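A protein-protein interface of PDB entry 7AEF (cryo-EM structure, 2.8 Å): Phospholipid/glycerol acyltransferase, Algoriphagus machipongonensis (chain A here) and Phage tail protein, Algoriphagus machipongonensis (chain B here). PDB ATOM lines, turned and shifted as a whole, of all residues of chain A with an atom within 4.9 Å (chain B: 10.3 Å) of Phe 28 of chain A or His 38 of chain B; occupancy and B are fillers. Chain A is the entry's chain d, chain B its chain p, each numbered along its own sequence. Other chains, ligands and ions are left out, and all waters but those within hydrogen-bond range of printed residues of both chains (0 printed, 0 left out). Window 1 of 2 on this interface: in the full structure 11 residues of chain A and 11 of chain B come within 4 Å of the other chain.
The backbone NH (N) of Phe 12 of chain A lies within hydrogen-bond range of the backbone carbonyl oxygen (O) of Gly 39 of chain B, 3.1 Å away. The backbone NH (N) of Ala 40 of chain B sits close to the backbone carbonyl oxygen (O) of Phe 12 of chain A (3.1 Å). The backbone carbonyl oxygen of Phe 28 of chain A lies within hydrogen-bond range of the backbone NH of Gly 39 of chain B (2.8 Å).
NH2 of Arg 37 of chain B lies within hydrogen-bond range of O of Gly 39 of chain B (3.3 Å).
His 38 of chain B touches Glu 27 of chain A. CA of His 38 of chain B touches O of Phe 28 of chain A (3.5 Å).
Of chain B, only His 38 and Gly 39 come within 4 Å of Phe 28 of chain A. His 38 of chain B touches two residues of chain A. No residue of chain B comes within 4 Å of Val 14 of chain A. No residue of chain B comes within 4 Å of Leu 66 of chain A. Of the printed residues of chain A, Gly 39 of chain B touches Phe 12 (3.1 Å) and Phe 28 (2.8 Å). Of the printed residues of chain B, Phe 12 of chain A touches Gly 39 (3.1 Å) and Ala 40 (3.1 Å). Printed residues of chain A within 4 Å of Ala 40 of chain B: Phe 12 (3.1 Å). The nearest residue of chain B that does not touch Phe 28 of chain A is Ala 40 of chain B (4.7 Å). The nearest residue of chain A that does not touch His 38 of chain B is Gln 29 of chain A (4.7 Å). The nearest printed residue of chain B that does not touch Phe 12 of chain A is Ser 41 of chain B (5.5 Å).
Of the 12 printed residues of chain A, 3 touch a printed residue of chain B. Hydrophobic or aromatic side chains of chain A within 4 Å of the printed part of chain B: Phe 12. Hydrophobic or aromatic side chains of chain B within 4 Å of the printed part of chain A: His 38 and Ala 40. Among the printed residues, 5 pairs touch across the chains. Among the printed residues, no Asp or Glu carboxylate lies within 4 Å of a Lys or Arg side-chain nitrogen of the other chain.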
ATOM      1  N   PHE A  12     -16.049  -6.865   2.856  1.00  0.00           N
ATOM      2  CA  PHE A  12     -16.387  -8.199   2.364  1.00  0.00           C
ATOM      3  C   PHE A  12     -15.822  -9.324   3.246  1.00  0.00           C
ATOM      4  O   PHE A  12     -14.875  -9.121   4.003  1.00  0.00           O
ATOM      5  CB  PHE A  12     -15.874  -8.367   0.928  1.00  0.00           C
ATOM      6  CG  PHE A  12     -14.382  -8.139   0.784  1.00  0.00           C
ATOM      7  CD1 PHE A  12     -13.474  -9.173   0.925  1.00  0.00           C
ATOM      8  CD2 PHE A  12     -13.889  -6.881   0.503  1.00  0.00           C
ATOM      9  CE1 PHE A  12     -12.116  -8.938   0.824  1.00  0.00           C
ATOM     10  CE2 PHE A  12     -12.537  -6.660   0.385  1.00  0.00           C
ATOM     11  CZ  PHE A  12     -11.654  -7.696   0.538  1.00  0.00           C
ATOM     12  N   VAL A  14     -14.766 -13.824   3.231  1.00  0.00           N
ATOM     13  CA  VAL A  14     -14.556 -15.074   2.478  1.00  0.00           C
ATOM     14  C   VAL A  14     -14.731 -16.266   3.419  1.00  0.00           C
ATOM     15  O   VAL A  14     -14.017 -16.370   4.417  1.00  0.00           O
ATOM     16  CB  VAL A  14     -13.165 -15.114   1.824  1.00  0.00           C
ATOM     17  CG1 VAL A  14     -12.950 -16.430   1.080  1.00  0.00           C
ATOM     18  CG2 VAL A  14     -12.990 -13.931   0.897  1.00  0.00           C
ATOM     19  N   PHE A  16     -15.201 -20.658   3.885  1.00  0.00           N
ATOM     20  CA  PHE A  16     -14.872 -21.946   3.300  1.00  0.00           C
ATOM     21  C   PHE A  16     -15.749 -23.029   3.910  1.00  0.00           C
ATOM     22  O   PHE A  16     -16.005 -23.013   5.110  1.00  0.00           O
ATOM     23  CB  PHE A  16     -13.407 -22.294   3.575  1.00  0.00           C
ATOM     24  CG  PHE A  16     -12.409 -21.306   3.024  1.00  0.00           C
ATOM     25  CD1 PHE A  16     -12.097 -20.142   3.704  1.00  0.00           C
ATOM     26  CD2 PHE A  16     -11.749 -21.564   1.845  1.00  0.00           C
ATOM     27  CE1 PHE A  16     -11.190 -19.260   3.204  1.00  0.00           C
ATOM     28  CE2 PHE A  16     -10.828 -20.680   1.348  1.00  0.00           C
ATOM     29  CZ  PHE A  16     -10.553 -19.527   2.027  1.00  0.00           C
ATOM     30  N   ASP A  25      -8.737 -17.189   9.157  1.00  0.00           N
ATOM     31  CA  ASP A  25      -8.756 -17.606   7.764  1.00  0.00           C
ATOM     32  C   ASP A  25      -9.915 -16.989   6.990  1.00  0.00           C
ATOM     33  O   ASP A  25     -10.118 -17.333   5.828  1.00  0.00           O
ATOM     34  CB  ASP A  25      -8.802 -19.148   7.624  1.00  0.00           C
ATOM     35  CG  ASP A  25      -7.429 -19.866   7.855  1.00  0.00           C
ATOM     36  OD1 ASP A  25      -6.387 -19.392   7.390  1.00  0.00           O
ATOM     37  OD2 ASP A  25      -7.418 -20.955   8.457  1.00  0.00           O
ATOM     38  N   HIS A  26     -10.701 -16.114   7.602  1.00  0.00           N
ATOM     39  CA  HIS A  26     -11.784 -15.481   6.877  1.00  0.00           C
ATOM     40  C   HIS A  26     -11.460 -14.068   6.489  1.00  0.00           C
ATOM     41  O   HIS A  26     -12.297 -13.408   5.891  1.00  0.00           O
ATOM     42  CB  HIS A  26     -13.063 -15.463   7.694  1.00  0.00           C
ATOM     43  CG  HIS A  26     -13.593 -16.817   8.011  1.00  0.00           C
ATOM     44  ND1 HIS A  26     -13.273 -17.935   7.274  1.00  0.00           N
ATOM     45  CD2 HIS A  26     -14.439 -17.231   8.979  1.00  0.00           C
ATOM     46  CE1 HIS A  26     -13.893 -18.983   7.781  1.00  0.00           C
ATOM     47  NE2 HIS A  26     -14.606 -18.582   8.818  1.00  0.00           N
ATOM     48  N   GLU A  27     -10.275 -13.585   6.811  1.00  0.00           N
ATOM     49  CA  GLU A  27      -9.920 -12.197   6.566  1.00  0.00           C
ATOM     50  C   GLU A  27      -8.886 -12.049   5.459  1.00  0.00           C
ATOM     51  O   GLU A  27      -7.777 -12.571   5.566  1.00  0.00           O
ATOM     52  CB  GLU A  27      -9.403 -11.586   7.854  1.00  0.00           C
ATOM     53  CG  GLU A  27     -10.236 -11.996   9.037  1.00  0.00           C
ATOM     54  CD  GLU A  27      -9.537 -11.739  10.337  1.00  0.00           C
ATOM     55  OE1 GLU A  27      -8.325 -11.452  10.298  1.00  0.00           O
ATOM     56  OE2 GLU A  27     -10.195 -11.829  11.395  1.00  0.00           O
ATOM     57  N   PHE A  28      -9.229 -11.286   4.427  1.00  0.00           N
ATOM     58  CA  PHE A  28      -8.346 -11.119   3.288  1.00  0.00           C
ATOM     59  C   PHE A  28      -8.179  -9.660   2.907  1.00  0.00           C
ATOM     60  O   PHE A  28      -9.031  -8.818   3.173  1.00  0.00           O
ATOM     61  CB  PHE A  28      -8.842 -11.934   2.101  1.00  0.00           C
ATOM     62  CG  PHE A  28      -8.600 -13.395   2.255  1.00  0.00           C
ATOM     63  CD1 PHE A  28      -9.571 -14.225   2.794  1.00  0.00           C
ATOM     64  CD2 PHE A  28      -7.385 -13.935   1.906  1.00  0.00           C
ATOM     65  CE1 PHE A  28      -9.334 -15.568   2.956  1.00  0.00           C
ATOM     66  CE2 PHE A  28      -7.144 -15.270   2.068  1.00  0.00           C
ATOM     67  CZ  PHE A  28      -8.119 -16.088   2.593  1.00  0.00           C
ATOM     68  N   GLN A  29      -7.003  -9.382   2.350  1.00  0.00           N
ATOM     69  CA  GLN A  29      -6.661  -8.070   1.807  1.00  0.00           C
ATOM     70  C   GLN A  29      -7.349  -7.807   0.469  1.00  0.00           C
ATOM     71  O   GLN A  29      -7.780  -6.673   0.202  1.00  0.00           O
ATOM     72  CB  GLN A  29      -5.142  -7.966   1.643  1.00  0.00           C
ATOM     73  CG  GLN A  29      -4.672  -6.668   1.019  1.00  0.00           C
ATOM     74  CD  GLN A  29      -3.173  -6.608   0.836  1.00  0.00           C
ATOM     75  OE1 GLN A  29      -2.453  -7.520   1.231  1.00  0.00           O
ATOM     76  NE2 GLN A  29      -2.694  -5.526   0.236  1.00  0.00           N
ATOM     77  N   SER A  30      -7.454  -8.842  -0.385  1.00  0.00           N
ATOM     78  CA  SER A  30      -8.017  -8.637  -1.711  1.00  0.00           C
ATOM     79  C   SER A  30      -8.543  -9.954  -2.303  1.00  0.00           C
ATOM     80  O   SER A  30      -8.010 -11.036  -2.038  1.00  0.00           O
ATOM     81  CB  SER A  30      -6.966  -8.051  -2.638  1.00  0.00           C
ATOM     82  OG  SER A  30      -7.446  -8.038  -3.950  1.00  0.00           O
ATOM     83  N   LEU A  66      -6.778 -14.965  -3.980  1.00  0.00           N
ATOM     84  CA  LEU A  66      -6.875 -14.380  -2.649  1.00  0.00           C
ATOM     85  C   LEU A  66      -5.519 -13.904  -2.117  1.00  0.00           C
ATOM     86  O   LEU A  66      -4.525 -14.629  -2.198  1.00  0.00           O
ATOM     87  CB  LEU A  66      -7.469 -15.411  -1.685  1.00  0.00           C
ATOM     88  CG  LEU A  66      -8.852 -16.007  -2.007  1.00  0.00           C
ATOM     89  CD1 LEU A  66      -9.185 -17.112  -1.035  1.00  0.00           C
ATOM     90  CD2 LEU A  66      -9.898 -14.942  -1.925  1.00  0.00           C
ATOM     91  N   LYS A  67      -5.482 -12.710  -1.506  1.00  0.00           N
ATOM     92  CA  LYS A  67      -4.257 -12.198  -0.880  1.00  0.00           C
ATOM     93  C   LYS A  67      -4.471 -11.753   0.562  1.00  0.00           C
ATOM     94  O   LYS A  67      -5.545 -11.266   0.922  1.00  0.00           O
ATOM     95  CB  LYS A  67      -3.678 -11.018  -1.643  1.00  0.00           C
ATOM     96  CG  LYS A  67      -3.166 -11.363  -2.997  1.00  0.00           C
ATOM     97  CD  LYS A  67      -2.549 -10.161  -3.652  1.00  0.00           C
ATOM     98  CE  LYS A  67      -2.016 -10.496  -5.025  1.00  0.00           C
ATOM     99  NZ  LYS A  67      -1.467  -9.294  -5.719  1.00  0.00           N
ATOM    100  N   ARG A  68      -3.410 -11.886   1.371  1.00  0.00           N
ATOM    101  CA  ARG A  68      -3.396 -11.474   2.778  1.00  0.00           C
ATOM    102  C   ARG A  68      -1.969 -11.425   3.323  1.00  0.00           C
ATOM    103  O   ARG A  68      -1.039 -11.921   2.693  1.00  0.00           O
ATOM    104  CB  ARG A  68      -4.204 -12.434   3.625  1.00  0.00           C
ATOM    105  CG  ARG A  68      -3.594 -13.798   3.658  1.00  0.00           C
ATOM    106  CD  ARG A  68      -4.373 -14.693   4.493  1.00  0.00           C
ATOM    107  NE  ARG A  68      -3.690 -15.959   4.607  1.00  0.00           N
ATOM    108  CZ  ARG A  68      -4.183 -17.035   5.196  1.00  0.00           C
ATOM    109  NH1 ARG A  68      -5.394 -17.034   5.734  1.00  0.00           N
ATOM    110  NH2 ARG A  68      -3.430 -18.110   5.239  1.00  0.00           N
ATOM    111  N   GLU B  35       1.283   0.076   7.482  1.00  0.00           N
ATOM    112  CA  GLU B  35      -0.179   0.090   7.654  1.00  0.00           C
ATOM    113  C   GLU B  35      -0.882  -1.143   7.064  1.00  0.00           C
ATOM    114  O   GLU B  35      -0.457  -1.665   6.033  1.00  0.00           O
ATOM    115  CB  GLU B  35      -0.753   1.345   7.007  1.00  0.00           C
ATOM    116  CG  GLU B  35      -0.263   2.646   7.600  1.00  0.00           C
ATOM    117  CD  GLU B  35      -0.893   3.847   6.965  1.00  0.00           C
ATOM    118  OE1 GLU B  35      -1.576   3.671   5.987  1.00  0.00           O
ATOM    119  OE2 GLU B  35      -0.700   4.942   7.446  1.00  0.00           O
ATOM    120  N   TYR B  36      -2.002  -1.564   7.677  1.00  0.00           N
ATOM    121  CA  TYR B  36      -2.779  -2.718   7.178  1.00  0.00           C
ATOM    122  C   TYR B  36      -4.299  -2.723   7.456  1.00  0.00           C
ATOM    123  O   TYR B  36      -4.758  -2.284   8.509  1.00  0.00           O
ATOM    124  CB  TYR B  36      -2.178  -3.988   7.801  1.00  0.00           C
ATOM    125  CG  TYR B  36      -2.812  -5.306   7.404  1.00  0.00           C
ATOM    126  CD1 TYR B  36      -2.423  -5.945   6.252  1.00  0.00           C
ATOM    127  CD2 TYR B  36      -3.786  -5.873   8.203  1.00  0.00           C
ATOM    128  CE1 TYR B  36      -2.996  -7.143   5.909  1.00  0.00           C
ATOM    129  CE2 TYR B  36      -4.356  -7.064   7.858  1.00  0.00           C
ATOM    130  CZ  TYR B  36      -3.965  -7.701   6.720  1.00  0.00           C
ATOM    131  OH  TYR B  36      -4.531  -8.898   6.373  1.00  0.00           O
ATOM    132  N   ARG B  37      -5.100  -3.207   6.491  1.00  0.00           N
ATOM    133  CA  ARG B  37      -6.538  -3.428   6.713  1.00  0.00           C
ATOM    134  C   ARG B  37      -7.095  -4.622   5.933  1.00  0.00           C
ATOM    135  O   ARG B  37      -6.949  -4.693   4.716  1.00  0.00           O
ATOM    136  CB  ARG B  37      -7.400  -2.208   6.359  1.00  0.00           C
ATOM    137  CG  ARG B  37      -8.912  -2.453   6.567  1.00  0.00           C
ATOM    138  CD  ARG B  37      -9.827  -1.298   6.319  1.00  0.00           C
ATOM    139  NE  ARG B  37     -11.228  -1.737   6.556  1.00  0.00           N
ATOM    140  CZ  ARG B  37     -12.046  -2.324   5.624  1.00  0.00           C
ATOM    141  NH1 ARG B  37     -11.633  -2.472   4.380  1.00  0.00           N
ATOM    142  NH2 ARG B  37     -13.257  -2.771   5.938  1.00  0.00           N
ATOM    143  N   HIS B  38      -7.767  -5.544   6.610  1.00  0.00           N
ATOM    144  CA  HIS B  38      -8.405  -6.678   5.925  1.00  0.00           C
ATOM    145  C   HIS B  38      -9.870  -6.318   5.640  1.00  0.00           C
ATOM    146  O   HIS B  38     -10.528  -5.724   6.465  1.00  0.00           O
ATOM    147  CB  HIS B  38      -8.216  -8.026   6.631  1.00  0.00           C
ATOM    148  CG  HIS B  38      -8.825  -8.114   7.990  1.00  0.00           C
ATOM    149  ND1 HIS B  38     -10.037  -8.714   8.224  1.00  0.00           N
ATOM    150  CD2 HIS B  38      -8.378  -7.702   9.195  1.00  0.00           C
ATOM    151  CE1 HIS B  38     -10.329  -8.637   9.504  1.00  0.00           C
ATOM    152  NE2 HIS B  38      -9.329  -8.046  10.118  1.00  0.00           N
ATOM    153  N   GLY B  39     -10.351  -6.676   4.452  1.00  0.00           N
ATOM    154  CA  GLY B  39     -11.666  -6.312   3.933  1.00  0.00           C
ATOM    155  C   GLY B  39     -12.865  -6.534   4.855  1.00  0.00           C
ATOM    156  O   GLY B  39     -13.847  -5.798   4.760  1.00  0.00           O
ATOM    157  N   ALA B  40     -12.813  -7.527   5.734  1.00  0.00           N
ATOM    158  CA  ALA B  40     -13.934  -7.801   6.622  1.00  0.00           C
ATOM    159  C   ALA B  40     -13.974  -6.953   7.893  1.00  0.00           C
ATOM    160  O   ALA B  40     -14.892  -7.126   8.695  1.00  0.00           O
ATOM    161  CB  ALA B  40     -13.919  -9.261   7.017  1.00  0.00           C
ATOM    162  N   SER B  41     -12.992  -6.094   8.138  1.00  0.00           N
ATOM    163  CA  SER B  41     -12.997  -5.321   9.375  1.00  0.00           C
ATOM    164  C   SER B  41     -14.174  -4.328   9.482  1.00  0.00           C
ATOM    165  O   SER B  41     -14.469  -3.621   8.522  1.00  0.00           O
ATOM    166  CB  SER B  41     -11.720  -4.533   9.513  1.00  0.00           C
ATOM    167  OG  SER B  41     -11.773  -3.712  10.658  1.00  0.00           O
ATOM    168  N   PRO B  42     -14.864  -4.232  10.650  1.00  0.00           N
ATOM    169  CA  PRO B  42     -15.893  -3.251  10.984  1.00  0.00           C
ATOM    170  C   PRO B  42     -15.404  -1.799  10.971  1.00  0.00           C
ATOM    171  O   PRO B  42     -16.210  -0.875  10.949  1.00  0.00           O
ATOM    172  CB  PRO B  42     -16.286  -3.645  12.409  1.00  0.00           C
ATOM    173  CG  PRO B  42     -15.933  -5.073  12.526  1.00  0.00           C
ATOM    174  CD  PRO B  42     -14.708  -5.264  11.682  1.00  0.00           C
ATOM    175  N   GLU B  43     -14.090  -1.587  11.075  1.00  0.00           N
ATOM    176  CA  GLU B  43     -13.569  -0.230  11.049  1.00  0.00           C
ATOM    177  C   GLU B  43     -13.058   0.057   9.665  1.00  0.00           C
ATOM    178  O   GLU B  43     -12.477  -0.813   9.018  1.00  0.00           O
ATOM    179  CB  GLU B  43     -12.472  -0.001  12.085  1.00  0.00           C
ATOM    180  CG  GLU B  43     -12.941  -0.060  13.509  1.00  0.00           C
ATOM    181  CD  GLU B  43     -11.851   0.268  14.502  1.00  0.00           C
ATOM    182  OE1 GLU B  43     -10.716   0.305  14.107  1.00  0.00           O
ATOM    183  OE2 GLU B  43     -12.160   0.496  15.644  1.00  0.00           O
ATOM    184  N   TYR B  44     -13.183   1.301   9.247  1.00  0.00           N
ATOM    185  CA  TYR B  44     -12.799   1.692   7.909  1.00  0.00           C
ATOM    186  C   TYR B  44     -11.518   2.509   7.872  1.00  0.00           C
ATOM    187  O   TYR B  44     -11.375   3.442   7.088  1.00  0.00           O
ATOM    188  CB  TYR B  44     -13.977   2.395   7.260  1.00  0.00           C
ATOM    189  CG  TYR B  44     -15.237   1.525   7.362  1.00  0.00           C
ATOM    190  CD1 TYR B  44     -16.343   2.002   8.020  1.00  0.00           C
ATOM    191  CD2 TYR B  44     -15.254   0.233   6.868  1.00  0.00           C
ATOM    192  CE1 TYR B  44     -17.456   1.221   8.168  1.00  0.00           C
ATOM    193  CE2 TYR B  44     -16.363  -0.552   7.028  1.00  0.00           C
ATOM    194  CZ  TYR B  44     -17.465  -0.055   7.674  1.00  0.00           C
ATOM    195  OH  TYR B  44     -18.581  -0.830   7.835  1.00  0.00           O
ATOM    196  N   SER B  45     -10.593   2.139   8.740  1.00  0.00           N
ATOM    197  CA  SER B  45      -9.288   2.749   8.875  1.00  0.00           C
ATOM    198  C   SER B  45      -8.259   1.642   9.092  1.00  0.00           C
ATOM    199  O   SER B  45      -8.619   0.477   9.262  1.00  0.00           O
ATOM    200  CB  SER B  45      -9.287   3.741  10.014  1.00  0.00           C
ATOM    201  OG  SER B  45      -9.484   3.096  11.231  1.00  0.00           O
ATOM    202  N   LYS B  46      -6.977   1.984   9.040  1.00  0.00           N
ATOM    203  CA  LYS B  46      -5.908   0.986   9.143  1.00  0.00           C
ATOM    204  C   LYS B  46      -5.255   0.833  10.514  1.00  0.00           C
ATOM    205  O   LYS B  46      -5.253   1.755  11.326  1.00  0.00           O
ATOM    206  CB  LYS B  46      -4.849   1.338   8.109  1.00  0.00           C
ATOM    207  CG  LYS B  46      -5.365   1.254   6.690  1.00  0.00           C
ATOM    208  CD  LYS B  46      -4.338   1.629   5.697  1.00  0.00           C
ATOM    209  CE  LYS B  46      -4.882   1.591   4.303  1.00  0.00           C
ATOM    210  NZ  LYS B  46      -3.868   2.036   3.316  1.00  0.00           N
ATOM    211  N   ILE B  47      -4.642  -0.334  10.734  1.00  0.00           N
ATOM    212  CA  ILE B  47      -3.868  -0.611  11.945  1.00  0.00           C
ATOM    213  C   ILE B  47      -2.400  -0.330  11.656  1.00  0.00           C
ATOM    214  O   ILE B  47      -1.921  -0.551  10.541  1.00  0.00           O
ATOM    215  CB  ILE B  47      -4.083  -2.042  12.496  1.00  0.00           C
ATOM    216  CG1 ILE B  47      -3.637  -3.124  11.480  1.00  0.00           C
ATOM    217  CG2 ILE B  47      -5.558  -2.190  12.850  1.00  0.00           C
ATOM    218  CD1 ILE B  47      -3.572  -4.525  12.017  1.00  0.00           C
